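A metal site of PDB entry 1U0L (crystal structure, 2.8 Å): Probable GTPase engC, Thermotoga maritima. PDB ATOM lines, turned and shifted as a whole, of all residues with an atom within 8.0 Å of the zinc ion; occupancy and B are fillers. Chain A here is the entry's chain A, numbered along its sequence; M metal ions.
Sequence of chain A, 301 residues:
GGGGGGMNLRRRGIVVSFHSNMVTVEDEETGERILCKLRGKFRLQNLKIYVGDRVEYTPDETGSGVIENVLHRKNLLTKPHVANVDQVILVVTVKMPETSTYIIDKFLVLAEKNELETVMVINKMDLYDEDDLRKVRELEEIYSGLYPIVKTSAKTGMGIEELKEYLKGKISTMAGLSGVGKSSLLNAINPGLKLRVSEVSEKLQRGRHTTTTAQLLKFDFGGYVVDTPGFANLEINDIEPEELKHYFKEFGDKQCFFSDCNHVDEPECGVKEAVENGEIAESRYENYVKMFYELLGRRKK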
ATOM      1  N   LYS A 245     -20.540 -17.145 -19.118  1.00  0.00           N
ATOM      2  CA  LYS A 245     -21.469 -17.115 -17.983  1.00  0.00           C
ATOM      3  C   LYS A 245     -22.899 -16.686 -18.331  1.00  0.00           C
ATOM      4  O   LYS A 245     -23.843 -17.041 -17.626  1.00  0.00           O
ATOM      5  CB  LYS A 245     -20.916 -16.205 -16.875  1.00  0.00           C
ATOM      6  CG  LYS A 245     -21.107 -14.727 -17.168  1.00  0.00           C
ATOM      7  CD  LYS A 245     -20.461 -13.842 -16.134  1.00  0.00           C
ATOM      8  CE  LYS A 245     -18.950 -13.883 -16.242  1.00  0.00           C
ATOM      9  NZ  LYS A 245     -18.352 -12.641 -15.698  1.00  0.00           N
ATOM     10  N   PHE A 251     -27.232 -18.747 -14.044  1.00  0.00           N
ATOM     11  CA  PHE A 251     -26.338 -17.666 -13.671  1.00  0.00           C
ATOM     12  C   PHE A 251     -26.968 -16.360 -14.145  1.00  0.00           C
ATOM     13  O   PHE A 251     -26.874 -16.015 -15.330  1.00  0.00           O
ATOM     14  CB  PHE A 251     -24.964 -17.833 -14.341  1.00  0.00           C
ATOM     15  CG  PHE A 251     -24.305 -19.167 -14.111  1.00  0.00           C
ATOM     16  CD1 PHE A 251     -24.997 -20.233 -13.537  1.00  0.00           C
ATOM     17  CD2 PHE A 251     -22.987 -19.378 -14.508  1.00  0.00           C
ATOM     18  CE1 PHE A 251     -24.399 -21.460 -13.380  1.00  0.00           C
ATOM     19  CE2 PHE A 251     -22.381 -20.616 -14.352  1.00  0.00           C
ATOM     20  CZ  PHE A 251     -23.082 -21.653 -13.790  1.00  0.00           C
ATOM     21  N   LYS A 254     -28.497 -14.530  -9.641  1.00  0.00           N
ATOM     22  CA  LYS A 254     -27.522 -14.738  -8.576  1.00  0.00           C
ATOM     23  C   LYS A 254     -26.614 -13.503  -8.470  1.00  0.00           C
ATOM     24  O   LYS A 254     -26.162 -12.959  -9.488  1.00  0.00           O
ATOM     25  CB  LYS A 254     -26.682 -15.986  -8.868  1.00  0.00           C
ATOM     26  CG  LYS A 254     -26.657 -17.002  -7.741  1.00  0.00           C
ATOM     27  CD  LYS A 254     -27.969 -17.772  -7.609  1.00  0.00           C
ATOM     28  CE  LYS A 254     -28.250 -18.645  -8.826  1.00  0.00           C
ATOM     29  NZ  LYS A 254     -29.481 -19.487  -8.694  1.00  0.00           N
ATOM     30  N   GLN A 255     -26.351 -13.056  -7.236  1.00  0.00           N
ATOM     31  CA  GLN A 255     -25.498 -11.885  -7.012  1.00  0.00           C
ATOM     32  C   GLN A 255     -24.138 -12.261  -6.433  1.00  0.00           C
ATOM     33  O   GLN A 255     -24.046 -13.003  -5.438  1.00  0.00           O
ATOM     34  CB  GLN A 255     -26.181 -10.878  -6.077  1.00  0.00           C
ATOM     35  CG  GLN A 255     -27.110  -9.892  -6.779  1.00  0.00           C
ATOM     36  CD  GLN A 255     -28.147 -10.581  -7.632  1.00  0.00           C
ATOM     37  OE1 GLN A 255     -28.980 -11.334  -7.129  1.00  0.00           O
ATOM     38  NE2 GLN A 255     -28.118 -10.330  -8.932  1.00  0.00           N
ATOM     39  N   CYS A 256     -23.096 -11.742  -7.063  1.00  0.00           N
ATOM     40  CA  CYS A 256     -21.715 -11.999  -6.654  1.00  0.00           C
ATOM     41  C   CYS A 256     -21.050 -10.686  -6.232  1.00  0.00           C
ATOM     42  O   CYS A 256     -21.314  -9.632  -6.820  1.00  0.00           O
ATOM     43  CB  CYS A 256     -20.926 -12.611  -7.822  1.00  0.00           C
ATOM     44  SG  CYS A 256     -21.461 -14.255  -8.334  1.00  0.00           S
ATOM     45  N   PHE A 257     -20.184 -10.768  -5.229  1.00  0.00           N
ATOM     46  CA  PHE A 257     -19.490  -9.586  -4.723  1.00  0.00           C
ATOM     47  C   PHE A 257     -18.978  -8.687  -5.831  1.00  0.00           C
ATOM     48  O   PHE A 257     -19.453  -7.571  -6.004  1.00  0.00           O
ATOM     49  CB  PHE A 257     -18.322  -9.995  -3.837  1.00  0.00           C
ATOM     50  CG  PHE A 257     -17.589  -8.823  -3.245  1.00  0.00           C
ATOM     51  CD1 PHE A 257     -18.089  -8.156  -2.132  1.00  0.00           C
ATOM     52  CD2 PHE A 257     -16.409  -8.365  -3.830  1.00  0.00           C
ATOM     53  CE1 PHE A 257     -17.435  -7.057  -1.602  1.00  0.00           C
ATOM     54  CE2 PHE A 257     -15.746  -7.267  -3.302  1.00  0.00           C
ATOM     55  CZ  PHE A 257     -16.257  -6.608  -2.185  1.00  0.00           C
ATOM     56  N   PHE A 258     -17.997  -9.178  -6.598  1.00  0.00           N
ATOM     57  CA  PHE A 258     -17.390  -8.396  -7.662  1.00  0.00           C
ATOM     58  C   PHE A 258     -18.268  -8.084  -8.873  1.00  0.00           C
ATOM     59  O   PHE A 258     -19.232  -8.791  -9.158  1.00  0.00           O
ATOM     60  CB  PHE A 258     -16.111  -9.060  -8.149  1.00  0.00           C
ATOM     61  CG  PHE A 258     -15.023  -9.113  -7.116  1.00  0.00           C
ATOM     62  CD1 PHE A 258     -14.961 -10.163  -6.202  1.00  0.00           C
ATOM     63  CD2 PHE A 258     -14.065  -8.104  -7.031  1.00  0.00           C
ATOM     64  CE1 PHE A 258     -13.970 -10.205  -5.229  1.00  0.00           C
ATOM     65  CE2 PHE A 258     -13.071  -8.127  -6.061  1.00  0.00           C
ATOM     66  CZ  PHE A 258     -13.022  -9.177  -5.155  1.00  0.00           C
ATOM     67  N   ASP A 260     -19.159  -8.238 -12.419  1.00  0.00           N
ATOM     68  CA  ASP A 260     -18.904  -9.238 -13.448  1.00  0.00           C
ATOM     69  C   ASP A 260     -17.914 -10.284 -12.922  1.00  0.00           C
ATOM     70  O   ASP A 260     -16.751 -10.345 -13.331  1.00  0.00           O
ATOM     71  CB  ASP A 260     -18.350  -8.589 -14.719  1.00  0.00           C
ATOM     72  CG  ASP A 260     -18.207  -9.585 -15.865  1.00  0.00           C
ATOM     73  OD1 ASP A 260     -19.231 -10.208 -16.240  1.00  0.00           O
ATOM     74  OD2 ASP A 260     -17.091  -9.754 -16.392  1.00  0.00           O
ATOM     75  N   CYS A 261     -18.392 -11.098 -11.992  1.00  0.00           N
ATOM     76  CA  CYS A 261     -17.609 -12.157 -11.408  1.00  0.00           C
ATOM     77  C   CYS A 261     -17.809 -13.363 -12.316  1.00  0.00           C
ATOM     78  O   CYS A 261     -18.937 -13.724 -12.618  1.00  0.00           O
ATOM     79  CB  CYS A 261     -18.169 -12.466 -10.019  1.00  0.00           C
ATOM     80  SG  CYS A 261     -17.602 -13.988  -9.308  1.00  0.00           S
ATOM     81  N   ASN A 262     -16.709 -13.976 -12.762  1.00  0.00           N
ATOM     82  CA  ASN A 262     -16.791 -15.131 -13.646  1.00  0.00           C
ATOM     83  C   ASN A 262     -17.200 -16.426 -12.947  1.00  0.00           C
ATOM     84  O   ASN A 262     -17.304 -17.479 -13.568  1.00  0.00           O
ATOM     85  CB  ASN A 262     -15.455 -15.322 -14.365  1.00  0.00           C
ATOM     86  CG  ASN A 262     -15.152 -14.162 -15.319  1.00  0.00           C
ATOM     87  OD1 ASN A 262     -16.010 -13.734 -16.104  1.00  0.00           O
ATOM     88  ND2 ASN A 262     -13.918 -13.668 -15.275  1.00  0.00           N
ATOM     89  N   HIS A 263     -17.439 -16.331 -11.641  1.00  0.00           N
ATOM     90  CA  HIS A 263     -17.880 -17.470 -10.841  1.00  0.00           C
ATOM     91  C   HIS A 263     -16.878 -18.613 -10.670  1.00  0.00           C
ATOM     92  O   HIS A 263     -17.247 -19.701 -10.210  1.00  0.00           O
ATOM     93  CB  HIS A 263     -19.176 -18.027 -11.435  1.00  0.00           C
ATOM     94  CG  HIS A 263     -20.117 -16.972 -11.934  1.00  0.00           C
ATOM     95  ND1 HIS A 263     -20.784 -16.116 -11.086  1.00  0.00           N
ATOM     96  CD2 HIS A 263     -20.464 -16.604 -13.192  1.00  0.00           C
ATOM     97  CE1 HIS A 263     -21.509 -15.270 -11.790  1.00  0.00           C
ATOM     98  NE2 HIS A 263     -21.327 -15.549 -13.074  1.00  0.00           N
ATOM     99  N   VAL A 264     -15.612 -18.400 -11.021  1.00  0.00           N
ATOM    100  CA  VAL A 264     -14.618 -19.452 -10.861  1.00  0.00           C
ATOM    101  C   VAL A 264     -13.872 -19.305  -9.535  1.00  0.00           C
ATOM    102  O   VAL A 264     -14.269 -19.880  -8.528  1.00  0.00           O
ATOM    103  CB  VAL A 264     -13.570 -19.457 -12.001  1.00  0.00           C
ATOM    104  CG1 VAL A 264     -12.570 -20.594 -11.798  1.00  0.00           C
ATOM    105  CG2 VAL A 264     -14.264 -19.582 -13.344  1.00  0.00           C
ATOM    106  N   ASP A 265     -12.804 -18.500  -9.535  1.00  0.00           N
ATOM    107  CA  ASP A 265     -11.994 -18.274  -8.342  1.00  0.00           C
ATOM    108  C   ASP A 265     -12.521 -17.197  -7.418  1.00  0.00           C
ATOM    109  O   ASP A 265     -12.400 -17.307  -6.200  1.00  0.00           O
ATOM    110  CB  ASP A 265     -10.551 -17.904  -8.723  1.00  0.00           C
ATOM    111  CG  ASP A 265      -9.707 -19.120  -9.063  1.00  0.00           C
ATOM    112  OD1 ASP A 265      -9.902 -20.178  -8.425  1.00  0.00           O
ATOM    113  OD2 ASP A 265      -8.828 -19.015  -9.943  1.00  0.00           O
ATOM    114  N   GLU A 266     -13.108 -16.152  -8.001  1.00  0.00           N
ATOM    115  CA  GLU A 266     -13.643 -15.020  -7.230  1.00  0.00           C
ATOM    116  C   GLU A 266     -14.130 -15.330  -5.797  1.00  0.00           C
ATOM    117  O   GLU A 266     -14.974 -16.202  -5.556  1.00  0.00           O
ATOM    118  CB  GLU A 266     -14.743 -14.304  -8.012  1.00  0.00           C
ATOM    119  CG  GLU A 266     -14.266 -13.571  -9.275  1.00  0.00           C
ATOM    120  CD  GLU A 266     -14.220 -14.450 -10.517  1.00  0.00           C
ATOM    121  OE1 GLU A 266     -14.656 -15.620 -10.446  1.00  0.00           O
ATOM    122  OE2 GLU A 266     -13.758 -13.966 -11.581  1.00  0.00           O
ATOM    123  N   PRO A 267     -13.587 -14.578  -4.831  1.00  0.00           N
ATOM    124  CA  PRO A 267     -13.770 -14.554  -3.372  1.00  0.00           C
ATOM    125  C   PRO A 267     -15.176 -14.755  -2.828  1.00  0.00           C
ATOM    126  O   PRO A 267     -15.359 -15.360  -1.779  1.00  0.00           O
ATOM    127  CB  PRO A 267     -13.212 -13.194  -2.992  1.00  0.00           C
ATOM    128  CG  PRO A 267     -12.066 -13.065  -3.947  1.00  0.00           C
ATOM    129  CD  PRO A 267     -12.675 -13.491  -5.248  1.00  0.00           C
ATOM    130  N   GLU A 268     -16.164 -14.233  -3.529  1.00  0.00           N
ATOM    131  CA  GLU A 268     -17.532 -14.360  -3.057  1.00  0.00           C
ATOM    132  C   GLU A 268     -18.385 -14.467  -4.298  1.00  0.00           C
ATOM    133  O   GLU A 268     -18.383 -13.566  -5.143  1.00  0.00           O
ATOM    134  CB  GLU A 268     -17.927 -13.128  -2.255  1.00  0.00           C
ATOM    135  CG  GLU A 268     -19.333 -13.200  -1.677  1.00  0.00           C
ATOM    136  CD  GLU A 268     -19.743 -11.921  -0.972  1.00  0.00           C
ATOM    137  OE1 GLU A 268     -19.043 -11.491  -0.031  1.00  0.00           O
ATOM    138  OE2 GLU A 268     -20.774 -11.340  -1.376  1.00  0.00           O
ATOM    139  N   CYS A 269     -19.107 -15.565  -4.422  1.00  0.00           N
ATOM    140  CA  CYS A 269     -19.919 -15.749  -5.609  1.00  0.00           C
ATOM    141  C   CYS A 269     -21.301 -16.297  -5.323  1.00  0.00           C
ATOM    142  O   CYS A 269     -21.425 -17.378  -4.763  1.00  0.00           O
ATOM    143  CB  CYS A 269     -19.184 -16.701  -6.545  1.00  0.00           C
ATOM    144  SG  CYS A 269     -20.122 -17.113  -7.999  1.00  0.00           S
ATOM    145  N   GLY A 270     -22.333 -15.569  -5.708  1.00  0.00           N
ATOM    146  CA  GLY A 270     -23.687 -16.050  -5.481  1.00  0.00           C
ATOM    147  C   GLY A 270     -23.915 -17.354  -6.220  1.00  0.00           C
ATOM    148  O   GLY A 270     -24.691 -18.220  -5.789  1.00  0.00           O
ATOM    149  N   VAL A 271     -23.234 -17.486  -7.357  1.00  0.00           N
ATOM    150  CA  VAL A 271     -23.351 -18.680  -8.142  1.00  0.00           C
ATOM    151  C   VAL A 271     -22.653 -19.811  -7.389  1.00  0.00           C
ATOM    152  O   VAL A 271     -23.265 -20.855  -7.142  1.00  0.00           O
ATOM    153  CB  VAL A 271     -22.699 -18.515  -9.525  1.00  0.00           C
ATOM    154  CG1 VAL A 271     -22.585 -19.871 -10.191  1.00  0.00           C
ATOM    155  CG2 VAL A 271     -23.538 -17.579 -10.379  1.00  0.00           C
ATOM    156  N   LYS A 272     -21.398 -19.615  -7.002  1.00  0.00           N
ATOM    157  CA  LYS A 272     -20.703 -20.651  -6.241  1.00  0.00           C
ATOM    158  C   LYS A 272     -21.473 -20.976  -4.971  1.00  0.00           C
ATOM    159  O   LYS A 272     -21.542 -22.132  -4.561  1.00  0.00           O
ATOM    160  CB  LYS A 272     -19.275 -20.230  -5.903  1.00  0.00           C
ATOM    161  CG  LYS A 272     -18.336 -20.453  -7.075  1.00  0.00           C
ATOM    162  CD  LYS A 272     -16.965 -20.938  -6.630  1.00  0.00           C
ATOM    163  CE  LYS A 272     -16.090 -19.774  -6.264  1.00  0.00           C
ATOM    164  NZ  LYS A 272     -14.766 -20.243  -5.766  1.00  0.00           N
ATOM    165  N   GLU A 273     -22.085 -19.963  -4.349  1.00  0.00           N
ATOM    166  CA  GLU A 273     -22.873 -20.184  -3.142  1.00  0.00           C
ATOM    167  C   GLU A 273     -24.040 -21.097  -3.466  1.00  0.00           C
ATOM    168  O   GLU A 273     -24.270 -22.087  -2.766  1.00  0.00           O
ATOM    169  CB  GLU A 273     -23.395 -18.848  -2.592  1.00  0.00           C
ATOM    170  CG  GLU A 273     -24.347 -19.012  -1.412  1.00  0.00           C
ATOM    171  CD  GLU A 273     -24.936 -17.695  -0.957  1.00  0.00           C
ATOM    172  OE1 GLU A 273     -24.167 -16.804  -0.532  1.00  0.00           O
ATOM    173  OE2 GLU A 273     -26.175 -17.535  -1.013  1.00  0.00           O
ATOM    174  N   TYR A 285     -22.525 -26.196 -13.026  1.00  0.00           N
ATOM    175  CA  TYR A 285     -21.353 -25.432 -12.618  1.00  0.00           C
ATOM    176  C   TYR A 285     -20.064 -26.041 -13.189  1.00  0.00           C
ATOM    177  O   TYR A 285     -19.240 -25.358 -13.805  1.00  0.00           O
ATOM    178  CB  TYR A 285     -21.254 -25.372 -11.095  1.00  0.00           C
ATOM    179  CG  TYR A 285     -20.092 -24.511 -10.667  1.00  0.00           C
ATOM    180  CD1 TYR A 285     -20.150 -23.136 -10.813  1.00  0.00           C
ATOM    181  CD2 TYR A 285     -18.898 -25.079 -10.245  1.00  0.00           C
ATOM    182  CE1 TYR A 285     -19.055 -22.341 -10.567  1.00  0.00           C
ATOM    183  CE2 TYR A 285     -17.782 -24.296  -9.993  1.00  0.00           C
ATOM    184  CZ  TYR A 285     -17.867 -22.922 -10.163  1.00  0.00           C
ATOM    185  OH  TYR A 285     -16.763 -22.118  -9.972  1.00  0.00           O
ATOM    186  N   TYR A 288     -19.583 -25.671 -16.878  1.00  0.00           N
ATOM    187  CA  TYR A 288     -19.347 -24.259 -17.172  1.00  0.00           C
ATOM    188  C   TYR A 288     -17.889 -23.893 -16.886  1.00  0.00           C
ATOM    189  O   TYR A 288     -17.228 -23.232 -17.685  1.00  0.00           O
ATOM    190  CB  TYR A 288     -20.274 -23.363 -16.343  1.00  0.00           C
ATOM    191  CG  TYR A 288     -19.741 -21.944 -16.279  1.00  0.00           C
ATOM    192  CD1 TYR A 288     -19.609 -21.170 -17.444  1.00  0.00           C
ATOM    193  CD2 TYR A 288     -19.264 -21.418 -15.083  1.00  0.00           C
ATOM    194  CE1 TYR A 288     -19.001 -19.931 -17.414  1.00  0.00           C
ATOM    195  CE2 TYR A 288     -18.660 -20.165 -15.034  1.00  0.00           C
ATOM    196  CZ  TYR A 288     -18.523 -19.432 -16.194  1.00  0.00           C
ATOM    197  OH  TYR A 288     -17.883 -18.215 -16.149  1.00  0.00           O
HETATM  198 ZN    ZN M   1     -19.596 -15.154  -9.247  1.00  0.00          ZN
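SG of Cys 256 sits close to N of Gly 270 (3.1 Å).
The backbone NH (N) of His 263 is in hydrogen-bond range of the side-chain carboxylate (OE1) of Glu 266, at 3.1 Å.
The side-chain carboxylate of Glu 266 sits close to the side-chain sulfur of Cys 261.
The backbone carbonyl oxygen (O) of His 263 sits at hydrogen-bond distance from the side-chain hydroxyl (OH) of Tyr 285 (2.5 Å).
The side-chain sulfur (SG) of Cys 269 lies close to the backbone NH (N) of Lys 272 (3.0 Å).
SG of Cys 269 sits close to N of Val 271.
The backbone carbonyl oxygen (O) of Cys 261 sits at hydrogen-bond distance from the side-chain amino group (NZ) of Lys 245, 3.3 Å away.
Within 4 Å of the zinc ion: Cys 256, Cys 261, His 263 and Cys 269.
The nearest printed residue that does not touch the zinc ion is Gly 270 (4.5 Å).
The side-chain sulfur (SG) of Cys 256 is bound to the zinc ion, 2.3 Å away.
SG of Cys 261 is bound to the zinc ion (2.3 Å).
The zinc ion is bound by the side-chain sulfur (SG) of Cys 269 (2.4 Å).
ND1 of His 263 binds the zinc ion (2.4 Å).
The zinc ion has four donor atoms within binding distance.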
